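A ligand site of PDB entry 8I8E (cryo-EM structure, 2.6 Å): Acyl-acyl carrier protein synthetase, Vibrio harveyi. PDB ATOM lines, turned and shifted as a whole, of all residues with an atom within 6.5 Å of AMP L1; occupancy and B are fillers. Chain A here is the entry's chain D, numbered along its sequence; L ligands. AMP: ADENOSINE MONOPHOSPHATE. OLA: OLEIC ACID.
O of Gly 317 sits at hydrogen-bond distance from N6 of AMP L1, at 2.5 Å. The guanidinium group (NH1) of Arg 426 sits at hydrogen-bond distance from an oxygen (O3') of AMP L1 (2.6 Å). An oxygen (O2') of AMP L1 lies within hydrogen-bond range of the side-chain carboxylate of Asp 411 (2.7 Å). The backbone NH of Ala 298 sits at hydrogen-bond distance from a nitrogen (N1) of AMP L1, at 3.1 Å. An oxygen (O3P) of AMP L1 is in hydrogen-bond range of the backbone NH (N) of Ser 321 (3.3 Å). OG of Ser 321 lies within hydrogen-bond range of O3P of AMP L1 (3.1 Å). The side-chain hydroxyl (OG1) of Thr 175 lies within hydrogen-bond range of an oxygen (O3P) of AMP L1, 3.4 Å away.
The backbone carbonyl oxygen (O) of Ile 294 sits at hydrogen-bond distance from the backbone NH (N) of Gly 317 (3.0 Å). The guanidinium group of Arg 426 lies within salt-bridge range of the side-chain carboxylate of Asp 411. The guanidinium group (NH1) of Arg 426 lies within hydrogen-bond range of the backbone carbonyl oxygen (O) of Thr 409, at 3.4 Å. NE of Arg 426 sits at hydrogen-bond distance from O of Gly 410, at 3.1 Å. The side-chain carboxylate (OD2) of Asp 411 is in hydrogen-bond range of the side-chain hydroxyl (OH) of Tyr 318, at 3.0 Å. The side-chain hydroxyl (OG1) of Thr 409 lies close to the backbone NH (N) of Asp 411. OH of Tyr 318 lies within hydrogen-bond range of OG1 of Thr 409, 3.4 Å away.
O of Gly 295 lies close to N7 of AMP L1 (3.0 Å). A nitrogen (N7) of AMP L1 sits close to the backbone carbonyl oxygen of Gly 296, at 3.4 Å. Residues that only touch AMP L1: Ala 297 (3.7 Å), Tyr 318 (3.6 Å), Gly 319 (3.2 Å), Met 320 (3.3 Å) and Glu 322 (3.6 Å).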
ATOM      1  N   THR A 175       3.245 -18.895   3.407  1.00  0.00           N
ATOM      2  CA  THR A 175       3.911 -19.911   2.617  1.00  0.00           C
ATOM      3  C   THR A 175       4.347 -21.065   3.510  1.00  0.00           C
ATOM      4  O   THR A 175       4.871 -20.857   4.601  1.00  0.00           O
ATOM      5  CB  THR A 175       5.101 -19.341   1.856  1.00  0.00           C
ATOM      6  OG1 THR A 175       5.853 -20.401   1.258  1.00  0.00           O
ATOM      7  CG2 THR A 175       6.017 -18.549   2.790  1.00  0.00           C
ATOM      8  N   THR A 176       4.143 -22.286   3.028  1.00  0.00           N
ATOM      9  CA  THR A 176       4.382 -23.500   3.801  1.00  0.00           C
ATOM     10  C   THR A 176       5.657 -24.216   3.378  1.00  0.00           C
ATOM     11  O   THR A 176       5.694 -25.443   3.290  1.00  0.00           O
ATOM     12  CB  THR A 176       3.184 -24.438   3.690  1.00  0.00           C
ATOM     13  OG1 THR A 176       3.538 -25.741   4.170  1.00  0.00           O
ATOM     14  CG2 THR A 176       2.723 -24.550   2.240  1.00  0.00           C
ATOM     15  N   GLY A 177       6.723 -23.465   3.106  1.00  0.00           N
ATOM     16  CA  GLY A 177       7.976 -24.049   2.681  1.00  0.00           C
ATOM     17  C   GLY A 177       8.691 -24.836   3.766  1.00  0.00           C
ATOM     18  O   GLY A 177       8.068 -25.298   4.727  1.00  0.00           O
ATOM     19  N   HIS A 226      -2.716 -18.090  -3.944  1.00  0.00           N
ATOM     20  CA  HIS A 226      -1.325 -18.507  -3.727  1.00  0.00           C
ATOM     21  C   HIS A 226      -0.364 -17.321  -3.748  1.00  0.00           C
ATOM     22  O   HIS A 226       0.270 -17.009  -2.739  1.00  0.00           O
ATOM     23  CB  HIS A 226      -0.932 -19.554  -4.771  1.00  0.00           C
ATOM     24  CG  HIS A 226      -0.919 -20.950  -4.254  1.00  0.00           C
ATOM     25  ND1 HIS A 226      -0.272 -21.308  -3.081  1.00  0.00           N
ATOM     26  CD2 HIS A 226      -1.475 -22.091  -4.729  1.00  0.00           C
ATOM     27  CE1 HIS A 226      -0.429 -22.598  -2.868  1.00  0.00           C
ATOM     28  NE2 HIS A 226      -1.151 -23.094  -3.850  1.00  0.00           N
ATOM     29  N   VAL A 227      -0.232 -16.665  -4.896  1.00  0.00           N
ATOM     30  CA  VAL A 227       0.723 -15.568  -5.042  1.00  0.00           C
ATOM     31  C   VAL A 227       0.087 -14.368  -5.729  1.00  0.00           C
ATOM     32  O   VAL A 227       0.747 -13.671  -6.499  1.00  0.00           O
ATOM     33  CB  VAL A 227       1.984 -16.039  -5.792  1.00  0.00           C
ATOM     34  CG1 VAL A 227       2.803 -16.978  -4.913  1.00  0.00           C
ATOM     35  CG2 VAL A 227       1.596 -16.779  -7.030  1.00  0.00           C
ATOM     36  N   ILE A 294       3.295 -21.793 -17.855  1.00  0.00           N
ATOM     37  CA  ILE A 294       3.459 -22.812 -16.825  1.00  0.00           C
ATOM     38  C   ILE A 294       4.489 -22.311 -15.823  1.00  0.00           C
ATOM     39  O   ILE A 294       5.655 -22.124 -16.172  1.00  0.00           O
ATOM     40  CB  ILE A 294       3.889 -24.158 -17.427  1.00  0.00           C
ATOM     41  CG1 ILE A 294       2.912 -24.568 -18.528  1.00  0.00           C
ATOM     42  CG2 ILE A 294       3.958 -25.222 -16.364  1.00  0.00           C
ATOM     43  CD1 ILE A 294       1.482 -24.653 -18.076  1.00  0.00           C
ATOM     44  N   GLY A 295       4.069 -22.101 -14.580  1.00  0.00           N
ATOM     45  CA  GLY A 295       4.955 -21.511 -13.614  1.00  0.00           C
ATOM     46  C   GLY A 295       4.935 -22.167 -12.252  1.00  0.00           C
ATOM     47  O   GLY A 295       5.640 -21.738 -11.343  1.00  0.00           O
ATOM     48  N   GLY A 296       4.142 -23.222 -12.095  1.00  0.00           N
ATOM     49  CA  GLY A 296       4.081 -23.914 -10.833  1.00  0.00           C
ATOM     50  C   GLY A 296       5.425 -24.471 -10.399  1.00  0.00           C
ATOM     51  O   GLY A 296       6.017 -23.975  -9.449  1.00  0.00           O
ATOM     52  N   ALA A 297       5.894 -25.500 -11.107  1.00  0.00           N
ATOM     53  CA  ALA A 297       7.241 -26.019 -10.892  1.00  0.00           C
ATOM     54  C   ALA A 297       7.678 -26.941 -12.014  1.00  0.00           C
ATOM     55  O   ALA A 297       7.031 -27.967 -12.246  1.00  0.00           O
ATOM     56  CB  ALA A 297       7.319 -26.758  -9.552  1.00  0.00           C
ATOM     57  N   ALA A 298       8.762 -26.591 -12.709  1.00  0.00           N
ATOM     58  CA  ALA A 298       9.523 -27.531 -13.532  1.00  0.00           C
ATOM     59  C   ALA A 298       8.649 -28.185 -14.603  1.00  0.00           C
ATOM     60  O   ALA A 298       8.331 -29.377 -14.554  1.00  0.00           O
ATOM     61  CB  ALA A 298      10.206 -28.595 -12.660  1.00  0.00           C
ATOM     62  N   LEU A 299       8.237 -27.373 -15.566  1.00  0.00           N
ATOM     63  CA  LEU A 299       7.511 -27.872 -16.719  1.00  0.00           C
ATOM     64  C   LEU A 299       8.348 -28.934 -17.432  1.00  0.00           C
ATOM     65  O   LEU A 299       9.449 -28.618 -17.910  1.00  0.00           O
ATOM     66  CB  LEU A 299       7.179 -26.739 -17.670  1.00  0.00           C
ATOM     67  CG  LEU A 299       6.766 -27.108 -19.098  1.00  0.00           C
ATOM     68  CD1 LEU A 299       5.473 -27.904 -19.104  1.00  0.00           C
ATOM     69  CD2 LEU A 299       6.625 -25.860 -19.956  1.00  0.00           C
ATOM     70  N   ALA A 316       7.259 -21.094 -20.017  1.00  0.00           N
ATOM     71  CA  ALA A 316       7.460 -21.235 -18.582  1.00  0.00           C
ATOM     72  C   ALA A 316       7.759 -19.892 -17.919  1.00  0.00           C
ATOM     73  O   ALA A 316       8.061 -18.897 -18.569  1.00  0.00           O
ATOM     74  CB  ALA A 316       8.595 -22.214 -18.298  1.00  0.00           C
ATOM     75  N   GLY A 317       7.655 -19.901 -16.598  1.00  0.00           N
ATOM     76  CA  GLY A 317       7.964 -18.734 -15.794  1.00  0.00           C
ATOM     77  C   GLY A 317       8.303 -19.159 -14.394  1.00  0.00           C
ATOM     78  O   GLY A 317       7.951 -20.258 -13.957  1.00  0.00           O
ATOM     79  N   TYR A 318       8.997 -18.279 -13.681  1.00  0.00           N
ATOM     80  CA  TYR A 318       9.576 -18.620 -12.382  1.00  0.00           C
ATOM     81  C   TYR A 318       9.191 -17.575 -11.348  1.00  0.00           C
ATOM     82  O   TYR A 318       9.178 -16.376 -11.625  1.00  0.00           O
ATOM     83  CB  TYR A 318      11.091 -18.720 -12.498  1.00  0.00           C
ATOM     84  CG  TYR A 318      11.829 -18.890 -11.201  1.00  0.00           C
ATOM     85  CD1 TYR A 318      11.486 -19.881 -10.297  1.00  0.00           C
ATOM     86  CD2 TYR A 318      12.903 -18.066 -10.887  1.00  0.00           C
ATOM     87  CE1 TYR A 318      12.168 -20.030  -9.116  1.00  0.00           C
ATOM     88  CE2 TYR A 318      13.587 -18.205  -9.715  1.00  0.00           C
ATOM     89  CZ  TYR A 318      13.224 -19.189  -8.830  1.00  0.00           C
ATOM     90  OH  TYR A 318      13.918 -19.331  -7.659  1.00  0.00           O
ATOM     91  N   GLY A 319       8.869 -18.046 -10.147  1.00  0.00           N
ATOM     92  CA  GLY A 319       8.558 -17.153  -9.046  1.00  0.00           C
ATOM     93  C   GLY A 319       8.286 -17.947  -7.785  1.00  0.00           C
ATOM     94  O   GLY A 319       8.274 -19.181  -7.800  1.00  0.00           O
ATOM     95  N   MET A 320       8.079 -17.223  -6.690  1.00  0.00           N
ATOM     96  CA  MET A 320       7.729 -17.835  -5.414  1.00  0.00           C
ATOM     97  C   MET A 320       6.961 -16.820  -4.577  1.00  0.00           C
ATOM     98  O   MET A 320       6.714 -15.688  -5.003  1.00  0.00           O
ATOM     99  CB  MET A 320       8.965 -18.314  -4.668  1.00  0.00           C
ATOM    100  CG  MET A 320       9.879 -17.202  -4.208  1.00  0.00           C
ATOM    101  SD  MET A 320      11.578 -17.757  -4.059  1.00  0.00           S
ATOM    102  CE  MET A 320      11.733 -18.629  -5.601  1.00  0.00           C
ATOM    103  N   SER A 321       6.594 -17.235  -3.370  1.00  0.00           N
ATOM    104  CA  SER A 321       5.748 -16.405  -2.518  1.00  0.00           C
ATOM    105  C   SER A 321       6.433 -15.103  -2.123  1.00  0.00           C
ATOM    106  O   SER A 321       5.793 -14.052  -2.035  1.00  0.00           O
ATOM    107  CB  SER A 321       5.342 -17.187  -1.268  1.00  0.00           C
ATOM    108  OG  SER A 321       4.550 -18.310  -1.606  1.00  0.00           O
ATOM    109  N   GLU A 322       7.740 -15.159  -1.871  1.00  0.00           N
ATOM    110  CA  GLU A 322       8.474 -13.990  -1.387  1.00  0.00           C
ATOM    111  C   GLU A 322       8.833 -12.999  -2.482  1.00  0.00           C
ATOM    112  O   GLU A 322       9.327 -11.917  -2.156  1.00  0.00           O
ATOM    113  CB  GLU A 322       9.749 -14.439  -0.672  1.00  0.00           C
ATOM    114  CG  GLU A 322       9.512 -15.254   0.586  1.00  0.00           C
ATOM    115  CD  GLU A 322       9.441 -16.745   0.321  1.00  0.00           C
ATOM    116  OE1 GLU A 322       8.871 -17.151  -0.707  1.00  0.00           O
ATOM    117  OE2 GLU A 322       9.968 -17.527   1.148  1.00  0.00           O
ATOM    118  N   SER A 349      11.040 -24.942 -21.956  1.00  0.00           N
ATOM    119  CA  SER A 349      10.993 -25.567 -20.651  1.00  0.00           C
ATOM    120  C   SER A 349      11.941 -24.924 -19.646  1.00  0.00           C
ATOM    121  O   SER A 349      11.869 -25.265 -18.455  1.00  0.00           O
ATOM    122  CB  SER A 349      11.322 -27.065 -20.762  1.00  0.00           C
ATOM    123  OG  SER A 349      10.381 -27.738 -21.558  1.00  0.00           O
ATOM    124  N   LYS A 350      12.801 -24.019 -20.076  1.00  0.00           N
ATOM    125  CA  LYS A 350      13.778 -23.423 -19.186  1.00  0.00           C
ATOM    126  C   LYS A 350      13.097 -22.472 -18.198  1.00  0.00           C
ATOM    127  O   LYS A 350      11.910 -22.176 -18.284  1.00  0.00           O
ATOM    128  CB  LYS A 350      14.834 -22.663 -19.989  1.00  0.00           C
ATOM    129  CG  LYS A 350      15.803 -23.566 -20.733  1.00  0.00           C
ATOM    130  CD  LYS A 350      16.963 -22.772 -21.300  1.00  0.00           C
ATOM    131  CE  LYS A 350      18.065 -23.684 -21.792  1.00  0.00           C
ATOM    132  NZ  LYS A 350      17.923 -25.073 -21.274  1.00  0.00           N
ATOM    133  N   THR A 351      13.879 -22.017 -17.222  1.00  0.00           N
ATOM    134  CA  THR A 351      13.380 -21.049 -16.255  1.00  0.00           C
ATOM    135  C   THR A 351      13.108 -19.703 -16.918  1.00  0.00           C
ATOM    136  O   THR A 351      12.129 -19.024 -16.587  1.00  0.00           O
ATOM    137  CB  THR A 351      14.366 -20.927 -15.099  1.00  0.00           C
ATOM    138  OG1 THR A 351      14.373 -22.139 -14.341  1.00  0.00           O
ATOM    139  CG2 THR A 351      14.003 -19.780 -14.192  1.00  0.00           C
ATOM    140  N   THR A 409      16.550 -17.292  -2.687  1.00  0.00           N
ATOM    141  CA  THR A 409      15.367 -18.025  -3.130  1.00  0.00           C
ATOM    142  C   THR A 409      15.404 -19.507  -2.769  1.00  0.00           C
ATOM    143  O   THR A 409      14.388 -20.187  -2.918  1.00  0.00           O
ATOM    144  CB  THR A 409      15.212 -17.885  -4.647  1.00  0.00           C
ATOM    145  OG1 THR A 409      16.258 -18.595  -5.316  1.00  0.00           O
ATOM    146  CG2 THR A 409      15.259 -16.428  -5.055  1.00  0.00           C
ATOM    147  N   GLY A 410      16.546 -20.011  -2.299  1.00  0.00           N
ATOM    148  CA  GLY A 410      16.645 -21.418  -1.968  1.00  0.00           C
ATOM    149  C   GLY A 410      16.682 -22.358  -3.154  1.00  0.00           C
ATOM    150  O   GLY A 410      16.376 -23.535  -3.006  1.00  0.00           O
ATOM    151  N   ASP A 411      17.049 -21.849  -4.336  1.00  0.00           N
ATOM    152  CA  ASP A 411      17.108 -22.648  -5.546  1.00  0.00           C
ATOM    153  C   ASP A 411      18.506 -22.590  -6.148  1.00  0.00           C
ATOM    154  O   ASP A 411      19.158 -21.539  -6.095  1.00  0.00           O
ATOM    155  CB  ASP A 411      16.081 -22.163  -6.577  1.00  0.00           C
ATOM    156  CG  ASP A 411      14.674 -22.608  -6.256  1.00  0.00           C
ATOM    157  OD1 ASP A 411      14.379 -23.812  -6.381  1.00  0.00           O
ATOM    158  OD2 ASP A 411      13.862 -21.753  -5.856  1.00  0.00           O
ATOM    159  N   ILE A 423      17.158 -23.983 -13.579  1.00  0.00           N
ATOM    160  CA  ILE A 423      17.126 -24.385 -12.173  1.00  0.00           C
ATOM    161  C   ILE A 423      17.378 -25.886 -12.058  1.00  0.00           C
ATOM    162  O   ILE A 423      16.750 -26.692 -12.761  1.00  0.00           O
ATOM    163  CB  ILE A 423      15.785 -24.000 -11.542  1.00  0.00           C
ATOM    164  CG1 ILE A 423      15.799 -22.526 -11.144  1.00  0.00           C
ATOM    165  CG2 ILE A 423      15.490 -24.858 -10.323  1.00  0.00           C
ATOM    166  CD1 ILE A 423      14.551 -22.100 -10.436  1.00  0.00           C
ATOM    167  N   ARG A 426      16.582 -27.685  -5.296  1.00  0.00           N
ATOM    168  CA  ARG A 426      16.557 -26.843  -4.106  1.00  0.00           C
ATOM    169  C   ARG A 426      17.902 -26.874  -3.373  1.00  0.00           C
ATOM    170  O   ARG A 426      18.731 -27.761  -3.576  1.00  0.00           O
ATOM    171  CB  ARG A 426      15.444 -27.286  -3.162  1.00  0.00           C
ATOM    172  CG  ARG A 426      14.050 -27.150  -3.745  1.00  0.00           C
ATOM    173  CD  ARG A 426      13.663 -25.699  -3.904  1.00  0.00           C
ATOM    174  NE  ARG A 426      13.633 -24.996  -2.631  1.00  0.00           N
ATOM    175  CZ  ARG A 426      13.183 -23.766  -2.455  1.00  0.00           C
ATOM    176  NH1 ARG A 426      12.715 -23.050  -3.471  1.00  0.00           N
ATOM    177  NH2 ARG A 426      13.202 -23.223  -1.244  1.00  0.00           N
HETATM  178  P   AMP L   1       6.437 -21.118  -2.803  1.00  0.00           P
HETATM  179  O1P AMP L   1       5.521 -20.410  -3.728  1.00  0.00           O
HETATM  180  O2P AMP L   1       5.623 -22.114  -1.978  1.00  0.00           O
HETATM  181  O3P AMP L   1       7.105 -20.111  -1.870  1.00  0.00           O
HETATM  182  O5' AMP L   1       7.617 -21.948  -3.687  1.00  0.00           O
HETATM  183  C5' AMP L   1       7.756 -21.687  -5.037  1.00  0.00           C
HETATM  184  C4' AMP L   1       8.780 -22.686  -5.630  1.00  0.00           C
HETATM  185  O4' AMP L   1       8.301 -23.244  -6.751  1.00  0.00           O
HETATM  186  C3' AMP L   1      10.121 -21.923  -6.059  1.00  0.00           C
HETATM  187  O3' AMP L   1      11.003 -21.788  -4.936  1.00  0.00           O
HETATM  188  C2' AMP L   1      10.683 -22.691  -7.010  1.00  0.00           C
HETATM  189  O2' AMP L   1      11.661 -23.619  -6.411  1.00  0.00           O
HETATM  190  C1' AMP L   1       9.520 -23.476  -7.657  1.00  0.00           C
HETATM  191  N9  AMP L   1       9.292 -23.039  -8.904  1.00  0.00           N
HETATM  192  C8  AMP L   1       8.479 -22.056  -9.250  1.00  0.00           C
HETATM  193  N7  AMP L   1       8.504 -21.896 -10.568  1.00  0.00           N
HETATM  194  C5  AMP L   1       9.346 -22.798 -11.072  1.00  0.00           C
HETATM  195  C6  AMP L   1       9.766 -23.101 -12.340  1.00  0.00           C
HETATM  196  N6  AMP L   1       9.269 -22.371 -13.503  1.00  0.00           N
HETATM  197  N1  AMP L   1      10.648 -24.101 -12.482  1.00  0.00           N
HETATM  198  C2  AMP L   1      11.094 -24.758 -11.462  1.00  0.00           C
HETATM  199  N3  AMP L   1      10.707 -24.475 -10.227  1.00  0.00           N
HETATM  200  C4  AMP L   1       9.846 -23.526 -10.010  1.00  0.00           C
HETATM  201  C1  OLA L   2       0.261 -22.983  -7.551  1.00  0.00           C
HETATM  202  O1  OLA L   2      -0.637 -21.954  -7.828  1.00  0.00           O
HETATM  203  C2  OLA L   2       1.670 -22.420  -7.664  1.00  0.00           C
HETATM  204  C3  OLA L   2       1.948 -21.345  -6.612  1.00  0.00           C
HETATM  205  C4  OLA L   2       3.213 -21.646  -5.819  1.00  0.00           C
HETATM  206  C5  OLA L   2       4.495 -21.378  -6.602  1.00  0.00           C
HETATM  207  C6  OLA L   2       4.490 -20.010  -7.292  1.00  0.00           C
HETATM  208  C7  OLA L   2       4.538 -20.156  -8.818  1.00  0.00           C
HETATM  209  C8  OLA L   2       5.396 -19.095  -9.491  1.00  0.00           C
HETATM  210  C9  OLA L   2       4.569 -17.875  -9.884  1.00  0.00           C
HETATM  211  C10 OLA L   2       4.580 -17.419 -11.115  1.00  0.00           C
HETATM  212  C11 OLA L   2       5.407 -18.077 -12.208  1.00  0.00           C
HETATM  213  C12 OLA L   2       5.844 -17.049 -13.257  1.00  0.00           C
HETATM  214  C13 OLA L   2       4.927 -17.003 -14.468  1.00  0.00           C
HETATM  215  C14 OLA L   2       4.159 -15.686 -14.538  1.00  0.00           C
HETATM  216  C15 OLA L   2       3.274 -15.533 -15.766  1.00  0.00           C
HETATM  217  C16 OLA L   2       3.206 -14.110 -16.289  1.00  0.00           C
HETATM  218  C17 OLA L   2       2.622 -14.026 -17.691  1.00  0.00           C
HETATM  219  C18 OLA L   2       3.608 -14.452 -18.772  1.00  0.00           C
